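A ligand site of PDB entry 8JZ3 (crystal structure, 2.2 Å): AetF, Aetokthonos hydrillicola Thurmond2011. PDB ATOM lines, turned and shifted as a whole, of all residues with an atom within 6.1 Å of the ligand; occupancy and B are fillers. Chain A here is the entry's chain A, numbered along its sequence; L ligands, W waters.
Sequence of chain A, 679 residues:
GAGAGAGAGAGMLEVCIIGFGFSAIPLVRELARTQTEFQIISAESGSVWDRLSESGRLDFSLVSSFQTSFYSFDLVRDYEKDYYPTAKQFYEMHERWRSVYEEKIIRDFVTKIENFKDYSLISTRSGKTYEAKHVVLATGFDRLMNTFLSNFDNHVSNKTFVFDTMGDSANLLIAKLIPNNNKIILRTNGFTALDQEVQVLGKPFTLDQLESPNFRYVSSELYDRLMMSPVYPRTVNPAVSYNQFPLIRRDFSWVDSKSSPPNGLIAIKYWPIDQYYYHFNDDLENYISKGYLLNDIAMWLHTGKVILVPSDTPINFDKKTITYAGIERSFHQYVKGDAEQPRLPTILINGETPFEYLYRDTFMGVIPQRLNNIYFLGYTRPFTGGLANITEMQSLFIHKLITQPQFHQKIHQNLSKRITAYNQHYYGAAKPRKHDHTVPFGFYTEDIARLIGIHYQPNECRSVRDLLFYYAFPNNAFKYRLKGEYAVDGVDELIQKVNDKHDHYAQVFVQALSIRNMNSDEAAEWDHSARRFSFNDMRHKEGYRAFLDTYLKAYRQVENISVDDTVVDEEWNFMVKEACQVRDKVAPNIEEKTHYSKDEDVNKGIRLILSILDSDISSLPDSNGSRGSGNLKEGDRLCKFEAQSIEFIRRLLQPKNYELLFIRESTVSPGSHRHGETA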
ATOM      1  N   LEU A 194      27.583  -0.704  27.825  1.00  0.00           N
ATOM      2  CA  LEU A 194      28.277   0.229  26.889  1.00  0.00           C
ATOM      3  C   LEU A 194      29.629   0.582  27.501  1.00  0.00           C
ATOM      4  O   LEU A 194      29.671   1.069  28.623  1.00  0.00           O
ATOM      5  CB  LEU A 194      27.390   1.447  26.664  1.00  0.00           C
ATOM      6  CG  LEU A 194      26.077   1.176  25.950  1.00  0.00           C
ATOM      7  CD1 LEU A 194      25.108   2.347  26.094  1.00  0.00           C
ATOM      8  CD2 LEU A 194      26.312   0.882  24.485  1.00  0.00           C
ATOM      9  N   VAL A 198      35.984   4.961  24.922  1.00  0.00           N
ATOM     10  CA  VAL A 198      36.058   4.497  23.514  1.00  0.00           C
ATOM     11  C   VAL A 198      37.302   5.121  22.901  1.00  0.00           C
ATOM     12  O   VAL A 198      37.660   6.248  23.308  1.00  0.00           O
ATOM     13  CB  VAL A 198      34.725   4.837  22.827  1.00  0.00           C
ATOM     14  CG1 VAL A 198      34.829   5.027  21.333  1.00  0.00           C
ATOM     15  CG2 VAL A 198      33.689   3.781  23.163  1.00  0.00           C
ATOM     16  N   LEU A 207      31.977   7.809  26.395  1.00  0.00           N
ATOM     17  CA  LEU A 207      30.899   7.583  25.385  1.00  0.00           C
ATOM     18  C   LEU A 207      29.992   8.824  25.240  1.00  0.00           C
ATOM     19  O   LEU A 207      29.473   9.040  24.106  1.00  0.00           O
ATOM     20  CB  LEU A 207      30.089   6.315  25.731  1.00  0.00           C
ATOM     21  CG  LEU A 207      29.050   6.353  26.862  1.00  0.00           C
ATOM     22  CD1 LEU A 207      28.372   5.010  26.906  1.00  0.00           C
ATOM     23  CD2 LEU A 207      29.648   6.679  28.226  1.00  0.00           C
ATOM     24  N   ASP A 208      29.832   9.631  26.295  1.00  0.00           N
ATOM     25  CA  ASP A 208      28.982  10.852  26.324  1.00  0.00           C
ATOM     26  C   ASP A 208      29.511  11.952  25.387  1.00  0.00           C
ATOM     27  O   ASP A 208      28.709  12.818  25.003  1.00  0.00           O
ATOM     28  CB  ASP A 208      28.822  11.408  27.750  1.00  0.00           C
ATOM     29  CG  ASP A 208      30.136  11.732  28.432  1.00  0.00           C
ATOM     30  OD1 ASP A 208      30.810  10.748  28.883  1.00  0.00           O
ATOM     31  OD2 ASP A 208      30.476  12.934  28.504  1.00  0.00           O
ATOM     32  N   LEU A 210      30.291  11.491  22.339  1.00  0.00           N
ATOM     33  CA  LEU A 210      30.126  11.004  20.952  1.00  0.00           C
ATOM     34  C   LEU A 210      28.655  10.874  20.568  1.00  0.00           C
ATOM     35  O   LEU A 210      28.359  10.063  19.680  1.00  0.00           O
ATOM     36  CB  LEU A 210      30.809   9.643  20.856  1.00  0.00           C
ATOM     37  CG  LEU A 210      32.316   9.703  21.027  1.00  0.00           C
ATOM     38  CD1 LEU A 210      32.874   8.301  20.918  1.00  0.00           C
ATOM     39  CD2 LEU A 210      32.936  10.618  19.980  1.00  0.00           C
ATOM     40  N   GLU A 211      27.770  11.618  21.229  1.00  0.00           N
ATOM     41  CA  GLU A 211      26.291  11.444  21.133  1.00  0.00           C
ATOM     42  C   GLU A 211      25.721  12.525  20.217  1.00  0.00           C
ATOM     43  O   GLU A 211      24.602  12.314  19.720  1.00  0.00           O
ATOM     44  CB  GLU A 211      25.644  11.486  22.518  1.00  0.00           C
ATOM     45  CG  GLU A 211      26.057  10.306  23.369  1.00  0.00           C
ATOM     46  CD  GLU A 211      25.248  10.061  24.638  1.00  0.00           C
ATOM     47  OE1 GLU A 211      23.999  10.290  24.671  1.00  0.00           O
ATOM     48  OE2 GLU A 211      25.888   9.628  25.601  1.00  0.00           O
ATOM     49  N   SER A 212      26.445  13.631  20.039  1.00  0.00           N
ATOM     50  CA  SER A 212      26.029  14.752  19.163  1.00  0.00           C
ATOM     51  C   SER A 212      24.504  14.766  19.055  1.00  0.00           C
ATOM     52  O   SER A 212      23.928  14.611  17.973  1.00  0.00           O
ATOM     53  CB  SER A 212      26.660  14.604  17.827  1.00  0.00           C
ATOM     54  OG  SER A 212      26.157  13.430  17.210  1.00  0.00           O
ATOM     55  N   ARG A 225      20.335   5.961  13.362  1.00  0.00           N
ATOM     56  CA  ARG A 225      21.408   5.062  12.824  1.00  0.00           C
ATOM     57  C   ARG A 225      22.774   5.544  13.345  1.00  0.00           C
ATOM     58  O   ARG A 225      23.714   4.711  13.478  1.00  0.00           O
ATOM     59  CB  ARG A 225      21.281   4.901  11.305  1.00  0.00           C
ATOM     60  CG  ARG A 225      21.265   6.174  10.495  1.00  0.00           C
ATOM     61  CD  ARG A 225      21.029   5.817   9.036  1.00  0.00           C
ATOM     62  NE  ARG A 225      21.072   6.979   8.166  1.00  0.00           N
ATOM     63  CZ  ARG A 225      20.006   7.691   7.773  1.00  0.00           C
ATOM     64  NH1 ARG A 225      18.784   7.361   8.152  1.00  0.00           N
ATOM     65  NH2 ARG A 225      20.182   8.747   6.996  1.00  0.00           N
ATOM     66  N   LEU A 226      22.854   6.811  13.710  1.00  0.00           N
ATOM     67  CA  LEU A 226      23.967   7.433  14.472  1.00  0.00           C
ATOM     68  C   LEU A 226      24.167   6.642  15.766  1.00  0.00           C
ATOM     69  O   LEU A 226      25.300   6.439  16.152  1.00  0.00           O
ATOM     70  CB  LEU A 226      23.594   8.888  14.749  1.00  0.00           C
ATOM     71  CG  LEU A 226      24.682   9.947  14.943  1.00  0.00           C
ATOM     72  CD1 LEU A 226      25.341   9.835  16.306  1.00  0.00           C
ATOM     73  CD2 LEU A 226      25.714   9.917  13.820  1.00  0.00           C
ATOM     74  N   MET A 227      23.078   6.209  16.429  1.00  0.00           N
ATOM     75  CA  MET A 227      23.186   5.861  17.875  1.00  0.00           C
ATOM     76  C   MET A 227      22.896   4.400  18.178  1.00  0.00           C
ATOM     77  O   MET A 227      23.425   3.953  19.187  1.00  0.00           O
ATOM     78  CB  MET A 227      22.274   6.737  18.738  1.00  0.00           C
ATOM     79  CG  MET A 227      22.772   8.181  18.872  1.00  0.00           C
ATOM     80  SD  MET A 227      24.429   8.348  19.628  1.00  0.00           S
ATOM     81  CE  MET A 227      23.899   8.323  21.343  1.00  0.00           C
ATOM     82  N   MET A 228      22.049   3.690  17.426  1.00  0.00           N
ATOM     83  CA  MET A 228      21.298   2.558  18.029  1.00  0.00           C
ATOM     84  C   MET A 228      21.847   1.174  17.681  1.00  0.00           C
ATOM     85  O   MET A 228      21.360   0.212  18.336  1.00  0.00           O
ATOM     86  CB  MET A 228      19.822   2.638  17.648  1.00  0.00           C
ATOM     87  CG  MET A 228      19.141   3.840  18.229  1.00  0.00           C
ATOM     88  SD  MET A 228      19.300   3.921  20.024  1.00  0.00           S
ATOM     89  CE  MET A 228      18.316   2.514  20.530  1.00  0.00           C
ATOM     90  N   PRO A 230      24.677  -0.320  18.346  1.00  0.00           N
ATOM     91  CA  PRO A 230      25.238  -0.978  19.515  1.00  0.00           C
ATOM     92  C   PRO A 230      24.205  -1.426  20.558  1.00  0.00           C
ATOM     93  O   PRO A 230      24.593  -2.175  21.401  1.00  0.00           O
ATOM     94  CB  PRO A 230      26.195   0.043  20.145  1.00  0.00           C
ATOM     95  CG  PRO A 230      25.945   1.358  19.426  1.00  0.00           C
ATOM     96  CD  PRO A 230      24.900   1.130  18.350  1.00  0.00           C
ATOM     97  N   VAL A 231      22.939  -0.977  20.459  1.00  0.00           N
ATOM     98  CA  VAL A 231      21.879  -1.214  21.484  1.00  0.00           C
ATOM     99  C   VAL A 231      20.848  -2.195  20.889  1.00  0.00           C
ATOM    100  O   VAL A 231      20.603  -3.253  21.506  1.00  0.00           O
ATOM    101  CB  VAL A 231      21.205   0.100  21.925  1.00  0.00           C
ATOM    102  CG1 VAL A 231      20.189  -0.120  23.035  1.00  0.00           C
ATOM    103  CG2 VAL A 231      22.193   1.172  22.344  1.00  0.00           C
ATOM    104  N   PRO A 261      17.949   7.460  21.231  1.00  0.00           N
ATOM    105  CA  PRO A 261      17.511   6.338  22.057  1.00  0.00           C
ATOM    106  C   PRO A 261      16.286   6.747  22.868  1.00  0.00           C
ATOM    107  O   PRO A 261      16.101   7.928  23.137  1.00  0.00           O
ATOM    108  CB  PRO A 261      18.702   5.998  22.955  1.00  0.00           C
ATOM    109  CG  PRO A 261      19.628   7.168  22.838  1.00  0.00           C
ATOM    110  CD  PRO A 261      19.340   7.805  21.493  1.00  0.00           C
ATOM    111  N   PHE A 383      20.597   8.582  30.730  1.00  0.00           N
ATOM    112  CA  PHE A 383      20.903   7.317  30.024  1.00  0.00           C
ATOM    113  C   PHE A 383      22.395   7.047  30.142  1.00  0.00           C
ATOM    114  O   PHE A 383      22.806   5.923  30.422  1.00  0.00           O
ATOM    115  CB  PHE A 383      20.479   7.467  28.569  1.00  0.00           C
ATOM    116  CG  PHE A 383      20.927   6.361  27.664  1.00  0.00           C
ATOM    117  CD1 PHE A 383      20.763   5.027  28.036  1.00  0.00           C
ATOM    118  CD2 PHE A 383      21.428   6.638  26.402  1.00  0.00           C
ATOM    119  CE1 PHE A 383      21.170   4.002  27.202  1.00  0.00           C
ATOM    120  CE2 PHE A 383      21.799   5.612  25.548  1.00  0.00           C
ATOM    121  CZ  PHE A 383      21.642   4.297  25.943  1.00  0.00           C
ATOM    122  N   THR A 384      23.188   8.091  29.935  1.00  0.00           N
ATOM    123  CA  THR A 384      24.661   8.078  29.981  1.00  0.00           C
ATOM    124  C   THR A 384      25.158   9.382  30.587  1.00  0.00           C
ATOM    125  O   THR A 384      24.457  10.398  30.459  1.00  0.00           O
ATOM    126  CB  THR A 384      25.254   7.921  28.583  1.00  0.00           C
ATOM    127  OG1 THR A 384      24.964   9.130  27.878  1.00  0.00           O
ATOM    128  CG2 THR A 384      24.706   6.735  27.825  1.00  0.00           C
ATOM    129  N   VAL A 508      32.866  13.053  15.805  1.00  0.00           N
ATOM    130  CA  VAL A 508      31.426  12.659  15.861  1.00  0.00           C
ATOM    131  C   VAL A 508      30.663  13.384  14.762  1.00  0.00           C
ATOM    132  O   VAL A 508      29.727  12.789  14.235  1.00  0.00           O
ATOM    133  CB  VAL A 508      30.732  12.890  17.219  1.00  0.00           C
ATOM    134  CG1 VAL A 508      30.544  14.368  17.547  1.00  0.00           C
ATOM    135  CG2 VAL A 508      29.375  12.195  17.220  1.00  0.00           C
ATOM    136  N   GLN A 511      31.026  11.498  11.699  1.00  0.00           N
ATOM    137  CA  GLN A 511      30.233  10.245  11.748  1.00  0.00           C
ATOM    138  C   GLN A 511      28.853  10.514  11.142  1.00  0.00           C
ATOM    139  O   GLN A 511      28.335   9.683  10.375  1.00  0.00           O
ATOM    140  CB  GLN A 511      30.071   9.743  13.178  1.00  0.00           C
ATOM    141  CG  GLN A 511      29.155   8.535  13.285  1.00  0.00           C
ATOM    142  CD  GLN A 511      28.813   8.208  14.714  1.00  0.00           C
ATOM    143  OE1 GLN A 511      29.471   8.653  15.659  1.00  0.00           O
ATOM    144  NE2 GLN A 511      27.770   7.405  14.893  1.00  0.00           N
ATOM    145  N   TRP A 526      28.669  -0.394   9.067  1.00  0.00           N
ATOM    146  CA  TRP A 526      29.708   0.658   9.036  1.00  0.00           C
ATOM    147  C   TRP A 526      30.277   0.855  10.462  1.00  0.00           C
ATOM    148  O   TRP A 526      31.536   0.895  10.606  1.00  0.00           O
ATOM    149  CB  TRP A 526      29.102   1.940   8.449  1.00  0.00           C
ATOM    150  CG  TRP A 526      30.045   3.099   8.359  1.00  0.00           C
ATOM    151  CD1 TRP A 526      30.876   3.427   7.328  1.00  0.00           C
ATOM    152  CD2 TRP A 526      30.234   4.112   9.373  1.00  0.00           C
ATOM    153  NE1 TRP A 526      31.570   4.563   7.622  1.00  0.00           N
ATOM    154  CE2 TRP A 526      31.201   5.004   8.864  1.00  0.00           C
ATOM    155  CE3 TRP A 526      29.695   4.324  10.639  1.00  0.00           C
ATOM    156  CZ2 TRP A 526      31.629   6.101   9.605  1.00  0.00           C
ATOM    157  CZ3 TRP A 526      30.123   5.422  11.366  1.00  0.00           C
ATOM    158  CH2 TRP A 526      31.078   6.293  10.856  1.00  0.00           C
ATOM    159  N   ASP A 527      29.393   0.938  11.455  1.00  0.00           N
ATOM    160  CA  ASP A 527      29.758   1.188  12.879  1.00  0.00           C
ATOM    161  C   ASP A 527      30.672   0.081  13.381  1.00  0.00           C
ATOM    162  O   ASP A 527      31.515   0.355  14.277  1.00  0.00           O
ATOM    163  CB  ASP A 527      28.548   1.238  13.797  1.00  0.00           C
ATOM    164  CG  ASP A 527      27.904   2.609  13.822  1.00  0.00           C
ATOM    165  OD1 ASP A 527      28.663   3.618  14.004  1.00  0.00           O
ATOM    166  OD2 ASP A 527      26.667   2.651  13.683  1.00  0.00           O
ATOM    167  N   SER A 534      33.099   1.074  18.861  1.00  0.00           N
ATOM    168  CA  SER A 534      32.937   1.759  20.170  1.00  0.00           C
ATOM    169  C   SER A 534      32.618   0.772  21.320  1.00  0.00           C
ATOM    170  O   SER A 534      33.361   0.786  22.342  1.00  0.00           O
ATOM    171  CB  SER A 534      31.895   2.855  20.041  1.00  0.00           C
ATOM    172  OG  SER A 534      32.301   3.807  19.061  1.00  0.00           O
ATOM    173  N   PHE A 535      31.581  -0.054  21.171  1.00  0.00           N
ATOM    174  CA  PHE A 535      30.994  -0.841  22.297  1.00  0.00           C
ATOM    175  C   PHE A 535      30.990  -2.353  22.060  1.00  0.00           C
ATOM    176  O   PHE A 535      30.526  -2.872  20.981  1.00  0.00           O
ATOM    177  CB  PHE A 535      29.593  -0.334  22.577  1.00  0.00           C
ATOM    178  CG  PHE A 535      29.457   1.177  22.671  1.00  0.00           C
ATOM    179  CD1 PHE A 535      29.929   1.855  23.783  1.00  0.00           C
ATOM    180  CD2 PHE A 535      28.895   1.905  21.649  1.00  0.00           C
ATOM    181  CE1 PHE A 535      29.805   3.237  23.866  1.00  0.00           C
ATOM    182  CE2 PHE A 535      28.750   3.285  21.740  1.00  0.00           C
ATOM    183  CZ  PHE A 535      29.202   3.951  22.845  1.00  0.00           C
ATOM    184  N   LYS A 598      34.987   2.554   8.708  1.00  0.00           N
ATOM    185  CA  LYS A 598      34.736   3.630   9.695  1.00  0.00           C
ATOM    186  C   LYS A 598      36.027   4.432   9.925  1.00  0.00           C
ATOM    187  O   LYS A 598      35.940   5.684   9.911  1.00  0.00           O
ATOM    188  CB  LYS A 598      34.162   3.080  11.010  1.00  0.00           C
ATOM    189  CG  LYS A 598      33.962   4.112  12.105  1.00  0.00           C
ATOM    190  CD  LYS A 598      32.919   3.782  13.172  1.00  0.00           C
ATOM    191  CE  LYS A 598      33.057   4.652  14.405  1.00  0.00           C
ATOM    192  NZ  LYS A 598      31.871   4.576  15.284  1.00  0.00           N
HETATM  193  N1  LIG L   1      28.326   8.102  17.983  1.00  0.00           N
HETATM  194  C1  LIG L   1      29.290   7.136  18.665  1.00  0.00           C
HETATM  195  C2  LIG L   1      29.282   5.796  17.916  1.00  0.00           C
HETATM  196  O1  LIG L   1      28.448   5.653  17.009  1.00  0.00           O
HETATM  197  C3  LIG L   1      28.948   6.995  20.165  1.00  0.00           C
HETATM  198  C4  LIG L   1      27.672   6.310  20.505  1.00  0.00           C
HETATM  199  C5  LIG L   1      26.940   5.483  19.704  1.00  0.00           C
HETATM  200  C6  LIG L   1      26.996   6.308  21.774  1.00  0.00           C
HETATM  201  N2  LIG L   1      25.881   4.961  20.394  1.00  0.00           N
HETATM  202  C7  LIG L   1      25.885   5.443  21.659  1.00  0.00           C
HETATM  203  C8  LIG L   1      27.221   6.935  22.991  1.00  0.00           C
HETATM  204  C9  LIG L   1      24.996   5.209  22.706  1.00  0.00           C
HETATM  205  C10 LIG L   1      26.336   6.732  24.033  1.00  0.00           C
HETATM  206  C11 LIG L   1      25.260   5.863  23.881  1.00  0.00           C
HETATM  207  O2  LIG L   1      30.044   4.873  18.212  1.00  0.00           O
HETATM  208  O   HOH W   1      28.861   2.549  17.243  1.00  0.00           O
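O of Leu 226 lies close to O1 of the ligand (3.4 Å). Leu 207 touches the ligand (O to C8, 3.3 Å). Glu 211 touches the ligand (OE2 to C10, 3.3 Å). Pro 230 touches the ligand (CG to N2, 3.7 Å). Phe 383 touches the ligand. Asp 527 touches the ligand (OD1 to O1, 3.6 Å). Phe 535 touches the ligand. Hydrophobic or aromatic side chains within 4 Å of the ligand: Leu 207, Leu 210, Leu 226, Met 227, Pro 230, Phe 383 and Phe 535. 12 residues have an atom within 4 Å of the ligand: Leu 207, Leu 210, Glu 211, Leu 226, Met 227, Pro 230, Phe 383, Gln 511, Asp 527, Ser 534, Phe 535 and Lys 598. The nearest printed residue that does not touch the ligand is Thr 384 (4.1 Å).
The backbone carbonyl oxygen (O) of Leu 226 sits at hydrogen-bond distance from the side-chain amide nitrogen (NE2) of Gln 511 (2.9 Å). The side-chain carboxylate (OE2) of Glu 211 sits at hydrogen-bond distance from the side-chain hydroxyl (OG1) of Thr 384, at 2.5 Å. The side-chain carboxylate (OD1) of Asp 527 lies within salt-bridge range of the side-chain amino group (NZ) of Lys 598, 3.6 Å away.
A nitrogen (N1) of the ligand lies within hydrogen-bond range of the backbone carbonyl oxygen (O) of Leu 210 (2.6 Å). The side-chain hydroxyl (OG) of Ser 534 sits at hydrogen-bond distance from an oxygen (O2) of the ligand (2.6 Å). The side-chain amide oxygen (OE1) of Gln 511 sits at hydrogen-bond distance from a nitrogen (N1) of the ligand. O of Met 227 lies within hydrogen-bond range of N2 of the ligand (2.9 Å). SD of Met 227 sits close to N2 of the ligand (3.8 Å). The side-chain amino group of Lys 598 is in salt-bridge range of an oxygen (O2) of the ligand.
Water W1 bridges O2 of the ligand (2.8 Å) and OD1 of Asp 527 (3.4 Å).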
